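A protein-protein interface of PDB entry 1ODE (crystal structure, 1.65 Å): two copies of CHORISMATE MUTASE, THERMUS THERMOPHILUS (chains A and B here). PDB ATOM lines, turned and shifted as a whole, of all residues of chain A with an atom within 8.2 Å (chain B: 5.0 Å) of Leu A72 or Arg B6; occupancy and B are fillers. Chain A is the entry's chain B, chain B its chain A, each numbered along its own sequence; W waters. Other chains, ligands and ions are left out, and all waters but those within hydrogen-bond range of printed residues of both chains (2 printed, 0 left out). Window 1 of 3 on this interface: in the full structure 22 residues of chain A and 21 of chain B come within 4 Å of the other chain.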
ATOM      1  N   LEU A  27      11.376 -18.274 -33.757  1.00  0.00           N
ATOM      2  CA  LEU A  27      10.905 -19.296 -32.824  1.00  0.00           C
ATOM      3  C   LEU A  27       9.488 -19.744 -33.159  1.00  0.00           C
ATOM      4  O   LEU A  27       9.203 -20.939 -33.229  1.00  0.00           O
ATOM      5  CB  LEU A  27      10.956 -18.776 -31.383  1.00  0.00           C
ATOM      6  CG  LEU A  27      12.335 -18.670 -30.728  1.00  0.00           C
ATOM      7  CD1 LEU A  27      12.230 -17.915 -29.396  1.00  0.00           C
ATOM      8  CD2 LEU A  27      12.897 -20.079 -30.505  1.00  0.00           C
ATOM      9  N   LEU A  42       9.548 -29.284 -25.789  1.00  0.00           N
ATOM     10  CA  LEU A  42      10.914 -28.806 -25.947  1.00  0.00           C
ATOM     11  C   LEU A  42      11.811 -29.111 -24.758  1.00  0.00           C
ATOM     12  O   LEU A  42      11.601 -28.591 -23.663  1.00  0.00           O
ATOM     13  CB  LEU A  42      10.901 -27.302 -26.219  1.00  0.00           C
ATOM     14  CG  LEU A  42      10.072 -26.885 -27.434  1.00  0.00           C
ATOM     15  CD1 LEU A  42      10.081 -25.367 -27.553  1.00  0.00           C
ATOM     16  CD2 LEU A  42      10.639 -27.546 -28.696  1.00  0.00           C
ATOM     17  N   ALA A  43      12.816 -29.954 -24.985  1.00  0.00           N
ATOM     18  CA  ALA A  43      13.762 -30.310 -23.936  1.00  0.00           C
ATOM     19  C   ALA A  43      14.567 -29.074 -23.555  1.00  0.00           C
ATOM     20  O   ALA A  43      14.843 -28.836 -22.381  1.00  0.00           O
ATOM     21  CB  ALA A  43      14.706 -31.406 -24.428  1.00  0.00           C
ATOM     22  N   ALA A  44      14.943 -28.293 -24.565  1.00  0.00           N
ATOM     23  CA  ALA A  44      15.724 -27.082 -24.352  1.00  0.00           C
ATOM     24  C   ALA A  44      15.919 -26.371 -25.676  1.00  0.00           C
ATOM     25  O   ALA A  44      15.706 -26.948 -26.740  1.00  0.00           O
ATOM     26  CB  ALA A  44      17.088 -27.434 -23.757  1.00  0.00           C
ATOM     27  N   VAL A  45      16.332 -25.113 -25.606  1.00  0.00           N
ATOM     28  CA  VAL A  45      16.579 -24.335 -26.812  1.00  0.00           C
ATOM     29  C   VAL A  45      17.883 -23.583 -26.631  1.00  0.00           C
ATOM     30  O   VAL A  45      18.082 -22.883 -25.635  1.00  0.00           O
ATOM     31  CB  VAL A  45      15.449 -23.331 -27.091  1.00  0.00           C
ATOM     32  CG1 VAL A  45      15.751 -22.539 -28.364  1.00  0.00           C
ATOM     33  CG2 VAL A  45      14.131 -24.075 -27.236  1.00  0.00           C
ATOM     34  N   ILE A  46      18.773 -23.748 -27.601  1.00  0.00           N
ATOM     35  CA  ILE A  46      20.076 -23.105 -27.573  1.00  0.00           C
ATOM     36  C   ILE A  46      20.179 -22.077 -28.696  1.00  0.00           C
ATOM     37  O   ILE A  46      19.811 -22.353 -29.844  1.00  0.00           O
ATOM     38  CB  ILE A  46      21.188 -24.155 -27.739  1.00  0.00           C
ATOM     39  CG1 ILE A  46      21.076 -25.191 -26.613  1.00  0.00           C
ATOM     40  CG2 ILE A  46      22.557 -23.479 -27.744  1.00  0.00           C
ATOM     41  CD1 ILE A  46      22.001 -26.386 -26.782  1.00  0.00           C
ATOM     42  N   PHE A  47      20.674 -20.891 -28.356  1.00  0.00           N
ATOM     43  CA  PHE A  47      20.835 -19.817 -29.336  1.00  0.00           C
ATOM     44  C   PHE A  47      22.308 -19.463 -29.505  1.00  0.00           C
ATOM     45  O   PHE A  47      23.106 -19.635 -28.584  1.00  0.00           O
ATOM     46  CB  PHE A  47      20.129 -18.531 -28.882  1.00  0.00           C
ATOM     47  CG  PHE A  47      18.689 -18.701 -28.502  1.00  0.00           C
ATOM     48  CD1 PHE A  47      18.340 -19.219 -27.260  1.00  0.00           C
ATOM     49  CD2 PHE A  47      17.679 -18.285 -29.369  1.00  0.00           C
ATOM     50  CE1 PHE A  47      17.001 -19.320 -26.876  1.00  0.00           C
ATOM     51  CE2 PHE A  47      16.334 -18.381 -28.999  1.00  0.00           C
ATOM     52  CZ  PHE A  47      15.995 -18.899 -27.748  1.00  0.00           C
ATOM     53  N   PRO A  58      19.014 -13.081 -27.222  1.00  0.00           N
ATOM     54  CA  PRO A  58      17.850 -13.573 -27.967  1.00  0.00           C
ATOM     55  C   PRO A  58      16.874 -14.332 -27.068  1.00  0.00           C
ATOM     56  O   PRO A  58      15.679 -14.418 -27.361  1.00  0.00           O
ATOM     57  CB  PRO A  58      18.478 -14.476 -29.028  1.00  0.00           C
ATOM     58  CG  PRO A  58      19.797 -13.815 -29.284  1.00  0.00           C
ATOM     59  CD  PRO A  58      20.268 -13.489 -27.881  1.00  0.00           C
ATOM     60  N   ALA A  59      17.387 -14.884 -25.973  1.00  0.00           N
ATOM     61  CA  ALA A  59      16.557 -15.642 -25.045  1.00  0.00           C
ATOM     62  C   ALA A  59      15.383 -14.830 -24.511  1.00  0.00           C
ATOM     63  O   ALA A  59      14.345 -15.390 -24.171  1.00  0.00           O
ATOM     64  CB  ALA A  59      17.402 -16.170 -23.887  1.00  0.00           C
ATOM     65  N   GLU A  60      15.543 -13.512 -24.429  1.00  0.00           N
ATOM     66  CA  GLU A  60      14.462 -12.658 -23.941  1.00  0.00           C
ATOM     67  C   GLU A  60      13.213 -12.844 -24.800  1.00  0.00           C
ATOM     68  O   GLU A  60      12.090 -12.807 -24.297  1.00  0.00           O
ATOM     69  CB  GLU A  60      14.889 -11.189 -23.966  1.00  0.00           C
ATOM     70  CG  GLU A  60      15.959 -10.844 -22.954  1.00  0.00           C
ATOM     71  CD  GLU A  60      15.461 -10.978 -21.530  1.00  0.00           C
ATOM     72  OE1 GLU A  60      14.505 -10.259 -21.167  1.00  0.00           O
ATOM     73  OE2 GLU A  60      16.023 -11.801 -20.777  1.00  0.00           O
ATOM     74  N   ALA A  61      13.418 -13.049 -26.098  1.00  0.00           N
ATOM     75  CA  ALA A  61      12.314 -13.250 -27.035  1.00  0.00           C
ATOM     76  C   ALA A  61      11.513 -14.493 -26.669  1.00  0.00           C
ATOM     77  O   ALA A  61      10.290 -14.510 -26.783  1.00  0.00           O
ATOM     78  CB  ALA A  61      12.852 -13.374 -28.456  1.00  0.00           C
ATOM     79  N   ALA A  62      12.203 -15.541 -26.232  1.00  0.00           N
ATOM     80  CA  ALA A  62      11.527 -16.772 -25.846  1.00  0.00           C
ATOM     81  C   ALA A  62      10.611 -16.511 -24.649  1.00  0.00           C
ATOM     82  O   ALA A  62       9.514 -17.061 -24.568  1.00  0.00           O
ATOM     83  CB  ALA A  62      12.555 -17.849 -25.506  1.00  0.00           C
ATOM     84  N   ARG A  63      11.060 -15.671 -23.720  1.00  0.00           N
ATOM     85  CA  ARG A  63      10.245 -15.338 -22.552  1.00  0.00           C
ATOM     86  C   ARG A  63       8.997 -14.586 -23.021  1.00  0.00           C
ATOM     87  O   ARG A  63       7.885 -14.848 -22.557  1.00  0.00           O
ATOM     88  CB  ARG A  63      11.028 -14.455 -21.575  1.00  0.00           C
ATOM     89  CG  ARG A  63      10.167 -13.867 -20.457  1.00  0.00           C
ATOM     90  CD  ARG A  63      10.958 -12.949 -19.531  1.00  0.00           C
ATOM     91  NE  ARG A  63      11.560 -11.818 -20.236  1.00  0.00           N
ATOM     92  CZ  ARG A  63      10.876 -10.878 -20.882  1.00  0.00           C
ATOM     93  NH1 ARG A  63       9.548 -10.920 -20.923  1.00  0.00           N
ATOM     94  NH2 ARG A  63      11.521  -9.889 -21.487  1.00  0.00           N
ATOM     95  N   GLN A  64       9.197 -13.663 -23.956  1.00  0.00           N
ATOM     96  CA  GLN A  64       8.101 -12.856 -24.490  1.00  0.00           C
ATOM     97  C   GLN A  64       6.981 -13.708 -25.076  1.00  0.00           C
ATOM     98  O   GLN A  64       5.810 -13.354 -24.945  1.00  0.00           O
ATOM     99  CB  GLN A  64       8.633 -11.872 -25.542  1.00  0.00           C
ATOM    100  CG  GLN A  64       9.710 -10.932 -25.003  1.00  0.00           C
ATOM    101  CD  GLN A  64      10.309 -10.024 -26.067  1.00  0.00           C
ATOM    102  OE1 GLN A  64      10.421 -10.401 -27.232  1.00  0.00           O
ATOM    103  NE2 GLN A  64      10.720  -8.828 -25.660  1.00  0.00           N
ATOM    104  N   GLY A  66       6.177 -16.625 -24.037  1.00  0.00           N
ATOM    105  CA  GLY A  66       5.755 -17.584 -23.026  1.00  0.00           C
ATOM    106  C   GLY A  66       6.547 -18.859 -22.790  1.00  0.00           C
ATOM    107  O   GLY A  66       6.005 -19.822 -22.249  1.00  0.00           O
ATOM    108  N   MET A  67       7.821 -18.873 -23.169  1.00  0.00           N
ATOM    109  CA  MET A  67       8.651 -20.062 -22.978  1.00  0.00           C
ATOM    110  C   MET A  67       9.435 -20.050 -21.667  1.00  0.00           C
ATOM    111  O   MET A  67      10.550 -20.564 -21.603  1.00  0.00           O
ATOM    112  CB  MET A  67       9.631 -20.197 -24.142  1.00  0.00           C
ATOM    113  CG  MET A  67       8.973 -20.474 -25.474  1.00  0.00           C
ATOM    114  SD  MET A  67      10.212 -20.566 -26.783  1.00  0.00           S
ATOM    115  CE  MET A  67      10.968 -22.119 -26.419  1.00  0.00           C
ATOM    116  N   HIS A  68       8.848 -19.482 -20.619  1.00  0.00           N
ATOM    117  CA  HIS A  68       9.517 -19.404 -19.324  1.00  0.00           C
ATOM    118  C   HIS A  68       9.945 -20.749 -18.739  1.00  0.00           C
ATOM    119  O   HIS A  68      10.957 -20.824 -18.042  1.00  0.00           O
ATOM    120  CB  HIS A  68       8.630 -18.674 -18.307  1.00  0.00           C
ATOM    121  CG  HIS A  68       8.155 -17.331 -18.765  1.00  0.00           C
ATOM    122  ND1 HIS A  68       7.315 -17.168 -19.845  1.00  0.00           N
ATOM    123  CD2 HIS A  68       8.379 -16.091 -18.272  1.00  0.00           C
ATOM    124  CE1 HIS A  68       7.040 -15.884 -19.996  1.00  0.00           C
ATOM    125  NE2 HIS A  68       7.673 -15.210 -19.054  1.00  0.00           N
ATOM    126  N   ARG A  69       9.191 -21.808 -19.030  1.00  0.00           N
ATOM    127  CA  ARG A  69       9.515 -23.133 -18.498  1.00  0.00           C
ATOM    128  C   ARG A  69      10.416 -23.955 -19.417  1.00  0.00           C
ATOM    129  O   ARG A  69      10.729 -25.110 -19.121  1.00  0.00           O
ATOM    130  CB  ARG A  69       8.231 -23.915 -18.211  1.00  0.00           C
ATOM    131  CG  ARG A  69       7.444 -23.400 -17.015  1.00  0.00           C
ATOM    132  CD  ARG A  69       6.018 -23.919 -17.039  1.00  0.00           C
ATOM    133  NE  ARG A  69       5.298 -23.401 -18.200  1.00  0.00           N
ATOM    134  CZ  ARG A  69       4.019 -23.646 -18.467  1.00  0.00           C
ATOM    135  NH1 ARG A  69       3.302 -24.409 -17.653  1.00  0.00           N
ATOM    136  NH2 ARG A  69       3.455 -23.120 -19.546  1.00  0.00           N
ATOM    137  N   VAL A  70      10.824 -23.361 -20.533  1.00  0.00           N
ATOM    138  CA  VAL A  70      11.712 -24.041 -21.469  1.00  0.00           C
ATOM    139  C   VAL A  70      13.154 -23.668 -21.127  1.00  0.00           C
ATOM    140  O   VAL A  70      13.485 -22.486 -21.038  1.00  0.00           O
ATOM    141  CB  VAL A  70      11.433 -23.606 -22.920  1.00  0.00           C
ATOM    142  CG1 VAL A  70      12.381 -24.339 -23.877  1.00  0.00           C
ATOM    143  CG2 VAL A  70       9.974 -23.873 -23.270  1.00  0.00           C
ATOM    144  N   PRO A  71      14.027 -24.666 -20.905  1.00  0.00           N
ATOM    145  CA  PRO A  71      15.423 -24.338 -20.583  1.00  0.00           C
ATOM    146  C   PRO A  71      16.087 -23.674 -21.790  1.00  0.00           C
ATOM    147  O   PRO A  71      16.035 -24.202 -22.905  1.00  0.00           O
ATOM    148  CB  PRO A  71      16.040 -25.701 -20.272  1.00  0.00           C
ATOM    149  CG  PRO A  71      14.884 -26.487 -19.755  1.00  0.00           C
ATOM    150  CD  PRO A  71      13.765 -26.098 -20.692  1.00  0.00           C
ATOM    151  N   LEU A  72      16.706 -22.519 -21.565  1.00  0.00           N
ATOM    152  CA  LEU A  72      17.361 -21.775 -22.630  1.00  0.00           C
ATOM    153  C   LEU A  72      18.837 -21.545 -22.334  1.00  0.00           C
ATOM    154  O   LEU A  72      19.238 -21.411 -21.177  1.00  0.00           O
ATOM    155  CB  LEU A  72      16.676 -20.417 -22.801  1.00  0.00           C
ATOM    156  CG  LEU A  72      15.149 -20.407 -22.882  1.00  0.00           C
ATOM    157  CD1 LEU A  72      14.644 -18.966 -22.842  1.00  0.00           C
ATOM    158  CD2 LEU A  72      14.697 -21.102 -24.145  1.00  0.00           C
ATOM    159  N   LEU A  73      19.648 -21.509 -23.385  1.00  0.00           N
ATOM    160  CA  LEU A  73      21.072 -21.251 -23.230  1.00  0.00           C
ATOM    161  C   LEU A  73      21.567 -20.547 -24.494  1.00  0.00           C
ATOM    162  O   LEU A  73      21.135 -20.872 -25.598  1.00  0.00           O
ATOM    163  CB  LEU A  73      21.840 -22.562 -23.029  1.00  0.00           C
ATOM    164  CG  LEU A  73      23.297 -22.414 -22.584  1.00  0.00           C
ATOM    165  CD1 LEU A  73      23.333 -21.980 -21.114  1.00  0.00           C
ATOM    166  CD2 LEU A  73      24.042 -23.735 -22.755  1.00  0.00           C
ATOM    167  N   SER A  74      22.458 -19.573 -24.337  1.00  0.00           N
ATOM    168  CA  SER A  74      22.992 -18.864 -25.493  1.00  0.00           C
ATOM    169  C   SER A  74      24.514 -18.910 -25.533  1.00  0.00           C
ATOM    170  O   SER A  74      25.170 -19.079 -24.505  1.00  0.00           O
ATOM    171  CB  SER A  74      22.502 -17.413 -25.504  1.00  0.00           C
ATOM    172  OG  SER A  74      22.719 -16.789 -24.255  1.00  0.00           O
ATOM    173  N   ALA A  75      25.069 -18.775 -26.731  1.00  0.00           N
ATOM    174  CA  ALA A  75      26.511 -18.822 -26.900  1.00  0.00           C
ATOM    175  C   ALA A  75      26.941 -17.985 -28.097  1.00  0.00           C
ATOM    176  O   ALA A  75      26.119 -17.629 -28.937  1.00  0.00           O
ATOM    177  CB  ALA A  75      26.959 -20.261 -27.084  1.00  0.00           C
ATOM    178  N   VAL A  90      19.318 -20.857 -33.983  1.00  0.00           N
ATOM    179  CA  VAL A  90      18.624 -21.584 -32.930  1.00  0.00           C
ATOM    180  C   VAL A  90      18.692 -23.095 -33.137  1.00  0.00           C
ATOM    181  O   VAL A  90      18.659 -23.579 -34.267  1.00  0.00           O
ATOM    182  CB  VAL A  90      17.131 -21.165 -32.879  1.00  0.00           C
ATOM    183  CG1 VAL A  90      16.379 -21.981 -31.832  1.00  0.00           C
ATOM    184  CG2 VAL A  90      17.018 -19.673 -32.585  1.00  0.00           C
ATOM    185  N   LEU A  91      18.825 -23.823 -32.033  1.00  0.00           N
ATOM    186  CA  LEU A  91      18.824 -25.283 -32.050  1.00  0.00           C
ATOM    187  C   LEU A  91      17.882 -25.696 -30.935  1.00  0.00           C
ATOM    188  O   LEU A  91      18.216 -25.596 -29.755  1.00  0.00           O
ATOM    189  CB  LEU A  91      20.209 -25.880 -31.771  1.00  0.00           C
ATOM    190  CG  LEU A  91      20.174 -27.402 -31.538  1.00  0.00           C
ATOM    191  CD1 LEU A  91      19.696 -28.104 -32.810  1.00  0.00           C
ATOM    192  CD2 LEU A  91      21.553 -27.906 -31.140  1.00  0.00           C
ATOM    193  N   GLY B   4      15.816 -30.387 -20.041  1.00  0.00           N
ATOM    194  CA  GLY B   4      16.991 -29.603 -19.728  1.00  0.00           C
ATOM    195  C   GLY B   4      16.856 -29.047 -18.326  1.00  0.00           C
ATOM    196  O   GLY B   4      15.745 -28.805 -17.855  1.00  0.00           O
ATOM    197  N   ILE B   5      17.983 -28.889 -17.642  1.00  0.00           N
ATOM    198  CA  ILE B   5      17.992 -28.307 -16.309  1.00  0.00           C
ATOM    199  C   ILE B   5      18.945 -27.129 -16.389  1.00  0.00           C
ATOM    200  O   ILE B   5      20.090 -27.286 -16.810  1.00  0.00           O
ATOM    201  CB  ILE B   5      18.557 -29.240 -15.239  1.00  0.00           C
ATOM    202  CG1 ILE B   5      17.857 -30.596 -15.271  1.00  0.00           C
ATOM    203  CG2 ILE B   5      18.362 -28.601 -13.859  1.00  0.00           C
ATOM    204  CD1 ILE B   5      18.476 -31.582 -14.298  1.00  0.00           C
ATOM    205  N   ARG B   6      18.480 -25.953 -15.986  1.00  0.00           N
ATOM    206  CA  ARG B   6      19.329 -24.774 -16.023  1.00  0.00           C
ATOM    207  C   ARG B   6      19.883 -24.423 -14.654  1.00  0.00           C
ATOM    208  O   ARG B   6      19.227 -24.598 -13.628  1.00  0.00           O
ATOM    209  CB  ARG B   6      18.563 -23.562 -16.562  1.00  0.00           C
ATOM    210  CG  ARG B   6      18.510 -23.444 -18.089  1.00  0.00           C
ATOM    211  CD  ARG B   6      19.921 -23.373 -18.709  1.00  0.00           C
ATOM    212  NE  ARG B   6      20.824 -22.543 -17.916  1.00  0.00           N
ATOM    213  CZ  ARG B   6      20.781 -21.214 -17.846  1.00  0.00           C
ATOM    214  NH1 ARG B   6      19.879 -20.521 -18.535  1.00  0.00           N
ATOM    215  NH2 ARG B   6      21.623 -20.579 -17.045  1.00  0.00           N
ATOM    216  N   GLY B   7      21.109 -23.921 -14.658  1.00  0.00           N
ATOM    217  CA  GLY B   7      21.739 -23.506 -13.430  1.00  0.00           C
ATOM    218  C   GLY B   7      22.540 -22.262 -13.755  1.00  0.00           C
ATOM    219  O   GLY B   7      22.939 -22.059 -14.906  1.00  0.00           O
ATOM    220  N   ALA B   8      22.746 -21.413 -12.756  1.00  0.00           N
ATOM    221  CA  ALA B   8      23.545 -20.211 -12.936  1.00  0.00           C
ATOM    222  C   ALA B   8      24.054 -19.776 -11.574  1.00  0.00           C
ATOM    223  O   ALA B   8      23.335 -19.849 -10.577  1.00  0.00           O
ATOM    224  CB  ALA B   8      22.721 -19.094 -13.576  1.00  0.00           C
ATOM    225  N   MET B  30      21.803 -28.498  -8.334  1.00  0.00           N
ATOM    226  CA  MET B  30      20.951 -28.879  -9.458  1.00  0.00           C
ATOM    227  C   MET B  30      20.543 -30.341  -9.322  1.00  0.00           C
ATOM    228  O   MET B  30      19.391 -30.698  -9.564  1.00  0.00           O
ATOM    229  CB  MET B  30      21.691 -28.663 -10.779  1.00  0.00           C
ATOM    230  CG  MET B  30      21.821 -27.202 -11.158  1.00  0.00           C
ATOM    231  SD  MET B  30      22.902 -26.958 -12.570  1.00  0.00           S
ATOM    232  CE  MET B  30      21.823 -27.510 -13.915  1.00  0.00           C
ATOM    233  N   ARG B  89      27.026 -20.478 -16.260  1.00  0.00           N
ATOM    234  CA  ARG B  89      25.710 -21.024 -16.560  1.00  0.00           C
ATOM    235  C   ARG B  89      25.836 -22.484 -16.953  1.00  0.00           C
ATOM    236  O   ARG B  89      26.816 -22.884 -17.576  1.00  0.00           O
ATOM    237  CB  ARG B  89      25.047 -20.218 -17.681  1.00  0.00           C
ATOM    238  CG  ARG B  89      24.712 -18.776 -17.276  1.00  0.00           C
ATOM    239  CD  ARG B  89      24.090 -18.005 -18.432  1.00  0.00           C
ATOM    240  NE  ARG B  89      23.585 -16.685 -18.046  1.00  0.00           N
ATOM    241  CZ  ARG B  89      24.315 -15.573 -18.007  1.00  0.00           C
ATOM    242  NH1 ARG B  89      25.598 -15.601 -18.327  1.00  0.00           N
ATOM    243  NH2 ARG B  89      23.751 -14.423 -17.659  1.00  0.00           N
ATOM    244  N   VAL B  90      24.840 -23.280 -16.583  1.00  0.00           N
ATOM    245  CA  VAL B  90      24.863 -24.702 -16.881  1.00  0.00           C
ATOM    246  C   VAL B  90      23.554 -25.176 -17.493  1.00  0.00           C
ATOM    247  O   VAL B  90      22.477 -24.739 -17.080  1.00  0.00           O
ATOM    248  CB  VAL B  90      25.076 -25.543 -15.586  1.00  0.00           C
ATOM    249  CG1 VAL B  90      25.129 -27.030 -15.933  1.00  0.00           C
ATOM    250  CG2 VAL B  90      26.352 -25.114 -14.867  1.00  0.00           C
ATOM    251  N   LEU B  91      23.657 -26.050 -18.492  1.00  0.00           N
ATOM    252  CA  LEU B  91      22.486 -26.671 -19.102  1.00  0.00           C
ATOM    253  C   LEU B  91      22.723 -28.179 -19.083  1.00  0.00           C
ATOM    254  O   LEU B  91      23.546 -28.708 -19.842  1.00  0.00           O
ATOM    255  CB  LEU B  91      22.264 -26.228 -20.553  1.00  0.00           C
ATOM    256  CG  LEU B  91      21.152 -27.028 -21.269  1.00  0.00           C
ATOM    257  CD1 LEU B  91      19.796 -26.771 -20.602  1.00  0.00           C
ATOM    258  CD2 LEU B  91      21.092 -26.627 -22.742  1.00  0.00           C
ATOM    259  N   ARG B 104      13.386 -28.580 -11.685  1.00  0.00           N
ATOM    260  CA  ARG B 104      13.817 -27.478 -10.822  1.00  0.00           C
ATOM    261  C   ARG B 104      15.125 -26.844 -11.268  1.00  0.00           C
ATOM    262  O   ARG B 104      16.173 -27.492 -11.274  1.00  0.00           O
ATOM    263  CB  ARG B 104      13.989 -27.964  -9.379  1.00  0.00           C
ATOM    264  CG  ARG B 104      12.813 -28.746  -8.843  1.00  0.00           C
ATOM    265  CD  ARG B 104      11.523 -27.975  -8.996  1.00  0.00           C
ATOM    266  NE  ARG B 104      10.393 -28.729  -8.462  1.00  0.00           N
ATOM    267  CZ  ARG B 104       9.128 -28.522  -8.809  1.00  0.00           C
ATOM    268  NH1 ARG B 104       8.829 -27.581  -9.695  1.00  0.00           N
ATOM    269  NH2 ARG B 104       8.164 -29.261  -8.278  1.00  0.00           N
ATOM    270  N   HIS B 105      15.060 -25.564 -11.616  1.00  0.00           N
ATOM    271  CA  HIS B 105      16.239 -24.838 -12.060  1.00  0.00           C
ATOM    272  C   HIS B 105      16.829 -24.093 -10.875  1.00  0.00           C
ATOM    273  O   HIS B 105      16.109 -23.678  -9.965  1.00  0.00           O
ATOM    274  CB  HIS B 105      15.838 -23.925 -13.208  1.00  0.00           C
ATOM    275  CG  HIS B 105      15.096 -24.656 -14.285  1.00  0.00           C
ATOM    276  ND1 HIS B 105      15.703 -25.591 -15.095  1.00  0.00           N
ATOM    277  CD2 HIS B 105      13.777 -24.688 -14.598  1.00  0.00           C
ATOM    278  CE1 HIS B 105      14.792 -26.172 -15.857  1.00  0.00           C
ATOM    279  NE2 HIS B 105      13.614 -25.643 -15.573  1.00  0.00           N
ATOM    280  N   VAL B 106      18.148 -23.943 -10.886  1.00  0.00           N
ATOM    281  CA  VAL B 106      18.868 -23.333  -9.776  1.00  0.00           C
ATOM    282  C   VAL B 106      19.644 -22.063 -10.108  1.00  0.00           C
ATOM    283  O   VAL B 106      20.524 -22.062 -10.962  1.00  0.00           O
ATOM    284  CB  VAL B 106      19.840 -24.370  -9.170  1.00  0.00           C
ATOM    285  CG1 VAL B 106      20.541 -23.790  -7.958  1.00  0.00           C
ATOM    286  CG2 VAL B 106      19.072 -25.648  -8.804  1.00  0.00           C
ATOM    287  N   TYR B 107      19.317 -20.983  -9.406  1.00  0.00           N
ATOM    288  CA  TYR B 107      19.977 -19.697  -9.615  1.00  0.00           C
ATOM    289  C   TYR B 107      20.547 -19.257  -8.279  1.00  0.00           C
ATOM    290  O   TYR B 107      19.802 -18.975  -7.339  1.00  0.00           O
ATOM    291  CB  TYR B 107      18.961 -18.694 -10.157  1.00  0.00           C
ATOM    292  CG  TYR B 107      18.525 -19.057 -11.554  1.00  0.00           C
ATOM    293  CD1 TYR B 107      19.196 -18.552 -12.664  1.00  0.00           C
ATOM    294  CD2 TYR B 107      17.485 -19.959 -11.765  1.00  0.00           C
ATOM    295  CE1 TYR B 107      18.848 -18.939 -13.955  1.00  0.00           C
ATOM    296  CE2 TYR B 107      17.128 -20.353 -13.052  1.00  0.00           C
ATOM    297  CZ  TYR B 107      17.814 -19.840 -14.140  1.00  0.00           C
ATOM    298  OH  TYR B 107      17.471 -20.223 -15.418  1.00  0.00           O
HETATM  299  O   HOH W   1      11.604 -26.873 -17.233  1.00  0.00           O
HETATM  300  O   HOH W   2      12.607 -22.386 -16.338  1.00  0.00           O
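The backbone carbonyl oxygen of Ala A43 sits at hydrogen-bond distance from the backbone NH of Gly B4 (3.0 Å). The backbone carbonyl oxygen (O) of Leu A72 lies within hydrogen-bond range of the guanidinium group (NH1) of Arg B6.
The backbone NH (N) of Val B106 sits at hydrogen-bond distance from the backbone carbonyl oxygen (O) of Arg B6 (3.0 Å). The backbone carbonyl oxygen (O) of Val A45 is in hydrogen-bond range of the backbone NH (N) of Leu A73 (3.1 Å). The backbone NH (N) of Val A45 lies within hydrogen-bond range of the backbone carbonyl oxygen (O) of Pro A71 (2.9 Å). The backbone NH (N) of Phe A47 is in hydrogen-bond range of the backbone carbonyl oxygen (O) of Leu A73. N of Arg B6 sits at hydrogen-bond distance from ND1 of His B105 (2.9 Å). The guanidinium group of Arg B6 is in hydrogen-bond range of the backbone carbonyl oxygen of Val B90.
O of Gly B4 touches CG of Pro A71, 3.1 Å away. Arg B6 touches Pro A71 (CG to CB, 3.995 Å). Pro A71 touches Leu B91 (CB to CD1, 3.9 Å). His B105 touches Pro A71 (CE1 to CG, 3.9 Å). CB of Leu B91 touches CD2 of Leu A73, 3.8 Å away.
Pro A58 touches none of the printed residues of chain B. Glu A60 touches none of the printed residues of chain B. Of the printed residues of chain B, Leu A72 touches Arg B6 (2.9 Å). Printed residues of chain B within 4 Å of Leu A73: Leu B91 (3.8 Å). Of the printed residues of chain A, Gly B4 touches Ala A43 (3.0 Å) and Pro A71 (3.1 Å). Printed residues of chain A within 4 Å of Leu B91: Pro A71 (3.9 Å) and Leu A73 (3.8 Å). Printed residues of chain A within 4 Å of His B105: Pro A71.
Printed residues of chain A that touch a printed residue of chain B: Ala A43, Pro A71, Leu A72 and Leu A73. Hydrophobic or aromatic side chains of chain A that line the printed part of chain B: Pro A71 and Leu A73. Along chain A the printed residues that touch a printed residue of chain B span positions 43 to 73. Printed residues of chain B that touch a printed residue of chain A: Gly B4, Arg B6, Leu B91 and His B105. Among the printed residues, 7 pairs touch across the chains.
Positions printed for both chains: 90 and 91. Of the 7 pairs that touch across the chains among the printed residues, none has its exchanged pair printed and touching as well.
Water W1 lies within hydrogen-bond range of the backbone carbonyl oxygen of Arg A69 and a ring nitrogen (NE2) of His B105. Water W2 bridges O of His A68 and NE2 of His B105.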
